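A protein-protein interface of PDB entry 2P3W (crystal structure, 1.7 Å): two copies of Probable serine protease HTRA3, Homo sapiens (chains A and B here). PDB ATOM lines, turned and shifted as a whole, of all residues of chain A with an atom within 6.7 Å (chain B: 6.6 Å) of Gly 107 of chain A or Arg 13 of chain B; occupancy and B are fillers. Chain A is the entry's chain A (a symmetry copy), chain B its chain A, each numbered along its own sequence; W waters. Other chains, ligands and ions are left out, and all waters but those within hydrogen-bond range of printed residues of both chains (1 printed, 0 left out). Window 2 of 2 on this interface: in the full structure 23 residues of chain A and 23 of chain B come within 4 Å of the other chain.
Gly 107 of chain A touches just one residue of chain B: Arg 13.
Arg 13 of chain B touches just these residues of chain A: Gly 107 and Gly 109.
Of the printed residues of chain B, Gly 109 of chain A touches Met 12 and Arg 13.
Of the printed residues of chain A, Arg 11 of chain B touches Phe 108 (2.8 Å) and Arg 110 (3.5 Å).
Ile 37 of chain B touches none of the printed residues of chain A.
The nearest printed residue of chain A that does not touch Arg 11 of chain B is Gly 107 of chain A (4.6 Å).
The backbone NH (N) of Tyr 38 of chain B lies within hydrogen-bond range of the backbone carbonyl oxygen (O) of Arg 13 of chain B.
The side-chain hydroxyl (OG1) of Thr 14 of chain B is in hydrogen-bond range of the backbone NH (N) of Ser 70 of chain B (3.0 Å).
The guanidinium group (NH1) of Arg 13 of chain B sits at hydrogen-bond distance from the side-chain amide oxygen (OE1) of Gln 40 of chain B (3.0 Å).
The backbone carbonyl oxygen of Arg 11 of chain B lies within hydrogen-bond range of the backbone NH of Gln 40 of chain B (2.9 Å).
Among the printed residues, merely in contact across the chains: Gly 109 of chain A with Met 12 of chain B (3.2 Å), Gly 109 of chain A with Arg 13 of chain B (3.96 Å) and Arg 110 of chain A with Arg 11 of chain B (3.5 Å).
No position is printed for both chains.
Of the 7 pairs that touch across the chains among the printed residues, none has its exchanged pair printed and touching as well.
O of Arg 110 of chain A lies within hydrogen-bond range of N of Met 12 of chain B (2.9 Å).
The backbone carbonyl oxygen (O) of Phe 108 of chain A is in hydrogen-bond range of the guanidinium group (NH1) of Arg 11 of chain B, at 2.8 Å.
The backbone carbonyl oxygen (O) of Gly 107 of chain A sits at hydrogen-bond distance from the guanidinium group (NE) of Arg 13 of chain B (3.1 Å).
The side-chain hydroxyl of Ser 70 of chain B is in hydrogen-bond range of the guanidinium group of Arg 110 of chain A, 3.1 Å away.
Water W1 lies within hydrogen-bond range of OG of Ser 70 of chain B (3.0 Å), O of Met 12 of chain B (3.0 Å) and NH1 of Arg 110 of chain A (3.3 Å).
Printed residues of chain B that touch a printed residue of chain A: Arg 11, Met 12, Arg 13 and Ser 70.
Hydrophobic or aromatic side chains of chain B that line the printed part of chain A: Met 12.
Of the 9 printed residues of chain A, 4 touch a printed residue of chain B.
Hydrophobic or aromatic side chains of chain A that line the printed part of chain B: Phe 108.
Among the printed residues, no Asp or Glu carboxylate lies within 4 Å of a Lys or Arg side-chain nitrogen of the other chain.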
ATOM      1  N   HIS A   3      28.805  22.101  -5.497  1.00  0.00           N
ATOM      2  CA  HIS A   3      27.727  21.726  -4.602  1.00  0.00           C
ATOM      3  C   HIS A   3      28.214  20.797  -3.507  1.00  0.00           C
ATOM      4  O   HIS A   3      28.762  19.736  -3.801  1.00  0.00           O
ATOM      5  CB  HIS A   3      26.583  21.044  -5.373  1.00  0.00           C
ATOM      6  CG  HIS A   3      25.696  21.998  -6.121  1.00  0.00           C
ATOM      7  ND1 HIS A   3      26.088  22.628  -7.284  1.00  0.00           N
ATOM      8  CD2 HIS A   3      24.438  22.433  -5.864  1.00  0.00           C
ATOM      9  CE1 HIS A   3      25.108  23.411  -7.711  1.00  0.00           C
ATOM     10  NE2 HIS A   3      24.094  23.307  -6.869  1.00  0.00           N
ATOM     11  N   VAL A 103      30.750  15.726   0.985  1.00  0.00           N
ATOM     12  CA  VAL A 103      30.805  15.252  -0.409  1.00  0.00           C
ATOM     13  C   VAL A 103      30.674  16.447  -1.333  1.00  0.00           C
ATOM     14  O   VAL A 103      29.784  17.260  -1.184  1.00  0.00           O
ATOM     15  CB  VAL A 103      29.684  14.213  -0.711  1.00  0.00           C
ATOM     16  CG1 VAL A 103      29.843  13.622  -2.104  1.00  0.00           C
ATOM     17  CG2 VAL A 103      29.684  13.103   0.335  1.00  0.00           C
ATOM     18  N   MET A 104      31.569  16.517  -2.311  1.00  0.00           N
ATOM     19  CA  MET A 104      31.644  17.635  -3.233  1.00  0.00           C
ATOM     20  C   MET A 104      31.011  17.332  -4.595  1.00  0.00           C
ATOM     21  O   MET A 104      30.691  16.171  -4.932  1.00  0.00           O
ATOM     22  CB  MET A 104      33.107  18.009  -3.409  1.00  0.00           C
ATOM     23  CG  MET A 104      33.788  18.285  -2.110  1.00  0.00           C
ATOM     24  SD  MET A 104      35.468  18.778  -2.379  1.00  0.00           S
ATOM     25  CE  MET A 104      35.241  20.387  -3.149  1.00  0.00           C
ATOM     26  N   GLY A 105      30.805  18.380  -5.389  1.00  0.00           N
ATOM     27  CA  GLY A 105      30.483  18.180  -6.797  1.00  0.00           C
ATOM     28  C   GLY A 105      29.123  17.554  -7.048  1.00  0.00           C
ATOM     29  O   GLY A 105      28.861  17.014  -8.147  1.00  0.00           O
ATOM     30  N   GLY A 106      28.254  17.607  -6.038  1.00  0.00           N
ATOM     31  CA  GLY A 106      26.936  16.979  -6.117  1.00  0.00           C
ATOM     32  C   GLY A 106      26.945  15.467  -6.072  1.00  0.00           C
ATOM     33  O   GLY A 106      25.938  14.827  -6.410  1.00  0.00           O
ATOM     34  N   GLY A 107      28.065  14.889  -5.646  1.00  0.00           N
ATOM     35  CA  GLY A 107      28.223  13.433  -5.595  1.00  0.00           C
ATOM     36  C   GLY A 107      27.392  12.730  -4.533  1.00  0.00           C
ATOM     37  O   GLY A 107      27.371  11.498  -4.473  1.00  0.00           O
ATOM     38  N   PHE A 108      26.732  13.495  -3.674  1.00  0.00           N
ATOM     39  CA  PHE A 108      25.848  12.902  -2.642  1.00  0.00           C
ATOM     40  C   PHE A 108      24.608  12.260  -3.244  1.00  0.00           C
ATOM     41  O   PHE A 108      24.107  11.226  -2.777  1.00  0.00           O
ATOM     42  CB  PHE A 108      25.416  13.983  -1.674  1.00  0.00           C
ATOM     43  CG  PHE A 108      24.636  13.479  -0.487  1.00  0.00           C
ATOM     44  CD1 PHE A 108      25.245  12.741   0.515  1.00  0.00           C
ATOM     45  CD2 PHE A 108      23.268  13.758  -0.375  1.00  0.00           C
ATOM     46  CE1 PHE A 108      24.518  12.307   1.609  1.00  0.00           C
ATOM     47  CE2 PHE A 108      22.532  13.323   0.719  1.00  0.00           C
ATOM     48  CZ  PHE A 108      23.159  12.597   1.715  1.00  0.00           C
ATOM     49  N   GLY A 109      24.069  12.889  -4.271  1.00  0.00           N
ATOM     50  CA  GLY A 109      22.788  12.423  -4.823  1.00  0.00           C
ATOM     51  C   GLY A 109      21.644  12.795  -3.897  1.00  0.00           C
ATOM     52  O   GLY A 109      21.653  13.868  -3.289  1.00  0.00           O
ATOM     53  N   ARG A 110      20.650  11.917  -3.799  1.00  0.00           N
ATOM     54  CA  ARG A 110      19.589  12.107  -2.826  1.00  0.00           C
ATOM     55  C   ARG A 110      18.890  10.838  -2.438  1.00  0.00           C
ATOM     56  O   ARG A 110      18.796   9.916  -3.236  1.00  0.00           O
ATOM     57  CB  ARG A 110      18.553  13.113  -3.296  1.00  0.00           C
ATOM     58  CG  ARG A 110      17.755  12.740  -4.467  1.00  0.00           C
ATOM     59  CD  ARG A 110      16.727  13.865  -4.716  1.00  0.00           C
ATOM     60  NE  ARG A 110      15.968  13.655  -5.934  1.00  0.00           N
ATOM     61  CZ  ARG A 110      16.418  13.904  -7.162  1.00  0.00           C
ATOM     62  NH1 ARG A 110      17.650  14.349  -7.371  1.00  0.00           N
ATOM     63  NH2 ARG A 110      15.627  13.684  -8.201  1.00  0.00           N
ATOM     64  N   ARG B  11      19.928   5.866  -1.659  1.00  0.00           N
ATOM     65  CA  ARG B  11      20.504   7.164  -1.999  1.00  0.00           C
ATOM     66  C   ARG B  11      21.026   7.013  -3.439  1.00  0.00           C
ATOM     67  O   ARG B  11      21.866   6.169  -3.719  1.00  0.00           O
ATOM     68  CB  ARG B  11      21.578   7.582  -1.000  1.00  0.00           C
ATOM     69  CG  ARG B  11      22.179   8.943  -1.366  1.00  0.00           C
ATOM     70  CD  ARG B  11      22.544   9.784  -0.177  1.00  0.00           C
ATOM     71  NE  ARG B  11      23.572   9.180   0.666  1.00  0.00           N
ATOM     72  CZ  ARG B  11      24.858   9.163   0.377  1.00  0.00           C
ATOM     73  NH1 ARG B  11      25.290   9.701  -0.742  1.00  0.00           N
ATOM     74  NH2 ARG B  11      25.724   8.618   1.232  1.00  0.00           N
ATOM     75  N   MET B  12      20.421   7.770  -4.350  1.00  0.00           N
ATOM     76  CA  MET B  12      20.581   7.556  -5.770  1.00  0.00           C
ATOM     77  C   MET B  12      21.362   8.686  -6.409  1.00  0.00           C
ATOM     78  O   MET B  12      21.312   9.844  -5.959  1.00  0.00           O
ATOM     79  CB  MET B  12      19.197   7.423  -6.435  1.00  0.00           C
ATOM     80  CG  MET B  12      18.313   8.651  -6.320  1.00  0.00           C
ATOM     81  SD  MET B  12      16.778   8.579  -7.244  1.00  0.00           S
ATOM     82  CE  MET B  12      16.001  10.053  -6.698  1.00  0.00           C
ATOM     83  N   ARG B  13      22.105   8.353  -7.458  1.00  0.00           N
ATOM     84  CA  ARG B  13      22.871   9.303  -8.232  1.00  0.00           C
ATOM     85  C   ARG B  13      22.630   9.062  -9.727  1.00  0.00           C
ATOM     86  O   ARG B  13      22.643   7.911 -10.182  1.00  0.00           O
ATOM     87  CB  ARG B  13      24.361   9.097  -7.942  1.00  0.00           C
ATOM     88  CG  ARG B  13      24.762   9.439  -6.527  1.00  0.00           C
ATOM     89  CD  ARG B  13      26.211   9.104  -6.235  1.00  0.00           C
ATOM     90  NE  ARG B  13      27.155   9.850  -7.071  1.00  0.00           N
ATOM     91  CZ  ARG B  13      28.464   9.605  -7.155  1.00  0.00           C
ATOM     92  NH1 ARG B  13      29.029   8.592  -6.494  1.00  0.00           N
ATOM     93  NH2 ARG B  13      29.232  10.373  -7.922  1.00  0.00           N
ATOM     94  N   THR B  14      22.404  10.126 -10.495  1.00  0.00           N
ATOM     95  CA  THR B  14      22.294   9.998 -11.950  1.00  0.00           C
ATOM     96  C   THR B  14      23.622   9.559 -12.600  1.00  0.00           C
ATOM     97  O   THR B  14      24.666  10.162 -12.340  1.00  0.00           O
ATOM     98  CB  THR B  14      21.852  11.345 -12.586  1.00  0.00           C
ATOM     99  OG1 THR B  14      20.590  11.729 -12.032  1.00  0.00           O
ATOM    100  CG2 THR B  14      21.735  11.221 -14.095  1.00  0.00           C
ATOM    101  N   ILE B  15      23.573   8.524 -13.452  1.00  0.00           N
ATOM    102  CA  ILE B  15      24.744   8.123 -14.241  1.00  0.00           C
ATOM    103  C   ILE B  15      25.102   9.236 -15.228  1.00  0.00           C
ATOM    104  O   ILE B  15      24.272   9.661 -16.052  1.00  0.00           O
ATOM    105  CB  ILE B  15      24.505   6.803 -15.007  1.00  0.00           C
ATOM    106  CG1 ILE B  15      24.361   5.596 -14.044  1.00  0.00           C
ATOM    107  CG2 ILE B  15      25.612   6.568 -16.057  1.00  0.00           C
ATOM    108  CD1 ILE B  15      25.630   5.060 -13.471  1.00  0.00           C
ATOM    109  N   THR B  16      26.342   9.687 -15.127  1.00  0.00           N
ATOM    110  CA  THR B  16      26.926  10.676 -16.031  1.00  0.00           C
ATOM    111  C   THR B  16      28.229  10.095 -16.559  1.00  0.00           C
ATOM    112  O   THR B  16      28.739   9.121 -16.010  1.00  0.00           O
ATOM    113  CB  THR B  16      27.251  11.958 -15.266  1.00  0.00           C
ATOM    114  OG1 THR B  16      28.259  11.678 -14.286  1.00  0.00           O
ATOM    115  CG2 THR B  16      26.015  12.516 -14.587  1.00  0.00           C
ATOM    116  N   LEU B  19      30.804   9.847 -13.704  1.00  0.00           N
ATOM    117  CA  LEU B  19      30.593   8.663 -12.898  1.00  0.00           C
ATOM    118  C   LEU B  19      30.998   7.386 -13.653  1.00  0.00           C
ATOM    119  O   LEU B  19      31.612   6.491 -13.071  1.00  0.00           O
ATOM    120  CB  LEU B  19      29.122   8.617 -12.419  1.00  0.00           C
ATOM    121  CG  LEU B  19      28.705   7.565 -11.396  1.00  0.00           C
ATOM    122  CD1 LEU B  19      29.756   7.371 -10.324  1.00  0.00           C
ATOM    123  CD2 LEU B  19      27.372   7.938 -10.777  1.00  0.00           C
ATOM    124  N   GLU B  22      34.701   6.679 -13.292  1.00  0.00           N
ATOM    125  CA  GLU B  22      35.086   6.136 -11.981  1.00  0.00           C
ATOM    126  C   GLU B  22      34.757   4.655 -11.898  1.00  0.00           C
ATOM    127  O   GLU B  22      35.572   3.846 -11.453  1.00  0.00           O
ATOM    128  CB  GLU B  22      34.353   6.834 -10.842  1.00  0.00           C
ATOM    129  CG  GLU B  22      34.567   8.311 -10.759  1.00  0.00           C
ATOM    130  CD  GLU B  22      33.919   8.892  -9.528  1.00  0.00           C
ATOM    131  OE1 GLU B  22      33.539   8.103  -8.636  1.00  0.00           O
ATOM    132  OE2 GLU B  22      33.787  10.135  -9.443  1.00  0.00           O
ATOM    133  N   GLY B  36      21.358   5.528 -16.549  1.00  0.00           N
ATOM    134  CA  GLY B  36      20.599   4.915 -15.459  1.00  0.00           C
ATOM    135  C   GLY B  36      20.784   5.660 -14.137  1.00  0.00           C
ATOM    136  O   GLY B  36      21.287   6.797 -14.110  1.00  0.00           O
ATOM    137  N   ILE B  37      20.373   4.998 -13.063  1.00  0.00           N
ATOM    138  CA  ILE B  37      20.462   5.529 -11.711  1.00  0.00           C
ATOM    139  C   ILE B  37      21.374   4.666 -10.867  1.00  0.00           C
ATOM    140  O   ILE B  37      21.099   3.491 -10.636  1.00  0.00           O
ATOM    141  CB  ILE B  37      19.074   5.547 -11.019  1.00  0.00           C
ATOM    142  CG1 ILE B  37      18.010   6.247 -11.892  1.00  0.00           C
ATOM    143  CG2 ILE B  37      19.190   6.174  -9.659  1.00  0.00           C
ATOM    144  CD1 ILE B  37      18.376   7.577 -12.353  1.00  0.00           C
ATOM    145  N   TYR B  38      22.453   5.254 -10.369  1.00  0.00           N
ATOM    146  CA  TYR B  38      23.383   4.512  -9.515  1.00  0.00           C
ATOM    147  C   TYR B  38      22.939   4.457  -8.052  1.00  0.00           C
ATOM    148  O   TYR B  38      22.541   5.478  -7.469  1.00  0.00           O
ATOM    149  CB  TYR B  38      24.724   5.162  -9.610  1.00  0.00           C
ATOM    150  CG  TYR B  38      25.838   4.459  -8.857  1.00  0.00           C
ATOM    151  CD1 TYR B  38      26.403   3.288  -9.337  1.00  0.00           C
ATOM    152  CD2 TYR B  38      26.315   4.981  -7.678  1.00  0.00           C
ATOM    153  CE1 TYR B  38      27.435   2.648  -8.639  1.00  0.00           C
ATOM    154  CE2 TYR B  38      27.349   4.368  -6.972  1.00  0.00           C
ATOM    155  CZ  TYR B  38      27.898   3.200  -7.450  1.00  0.00           C
ATOM    156  OH  TYR B  38      28.933   2.609  -6.734  1.00  0.00           O
ATOM    157  N   VAL B  39      23.020   3.270  -7.456  1.00  0.00           N
ATOM    158  CA  VAL B  39      22.648   3.093  -6.046  1.00  0.00           C
ATOM    159  C   VAL B  39      23.894   3.301  -5.189  1.00  0.00           C
ATOM    160  O   VAL B  39      24.730   2.396  -5.021  1.00  0.00           O
ATOM    161  CB  VAL B  39      22.017   1.712  -5.767  1.00  0.00           C
ATOM    162  CG1 VAL B  39      21.609   1.581  -4.288  1.00  0.00           C
ATOM    163  CG2 VAL B  39      20.844   1.448  -6.697  1.00  0.00           C
ATOM    164  N   GLN B  40      24.005   4.519  -4.654  1.00  0.00           N
ATOM    165  CA  GLN B  40      25.123   4.880  -3.787  1.00  0.00           C
ATOM    166  C   GLN B  40      25.015   4.192  -2.432  1.00  0.00           C
ATOM    167  O   GLN B  40      26.010   3.696  -1.923  1.00  0.00           O
ATOM    168  CB  GLN B  40      25.213   6.406  -3.632  1.00  0.00           C
ATOM    169  CG  GLN B  40      26.334   6.908  -2.734  1.00  0.00           C
ATOM    170  CD  GLN B  40      27.735   6.638  -3.235  1.00  0.00           C
ATOM    171  OE1 GLN B  40      27.986   6.637  -4.428  1.00  0.00           O
ATOM    172  NE2 GLN B  40      28.683   6.489  -2.301  1.00  0.00           N
ATOM    173  N   SER B  70      17.721  10.852 -12.082  1.00  0.00           N
ATOM    174  CA  SER B  70      17.164  10.532 -10.765  1.00  0.00           C
ATOM    175  C   SER B  70      15.745  11.100 -10.547  1.00  0.00           C
ATOM    176  O   SER B  70      14.904  10.450  -9.898  1.00  0.00           O
ATOM    177  CB  SER B  70      18.125  10.978  -9.669  1.00  0.00           C
ATOM    178  OG  SER B  70      18.274  12.382  -9.668  1.00  0.00           O
HETATM  179  O   HOH W   1      20.206  12.277  -7.425  1.00  0.00           O
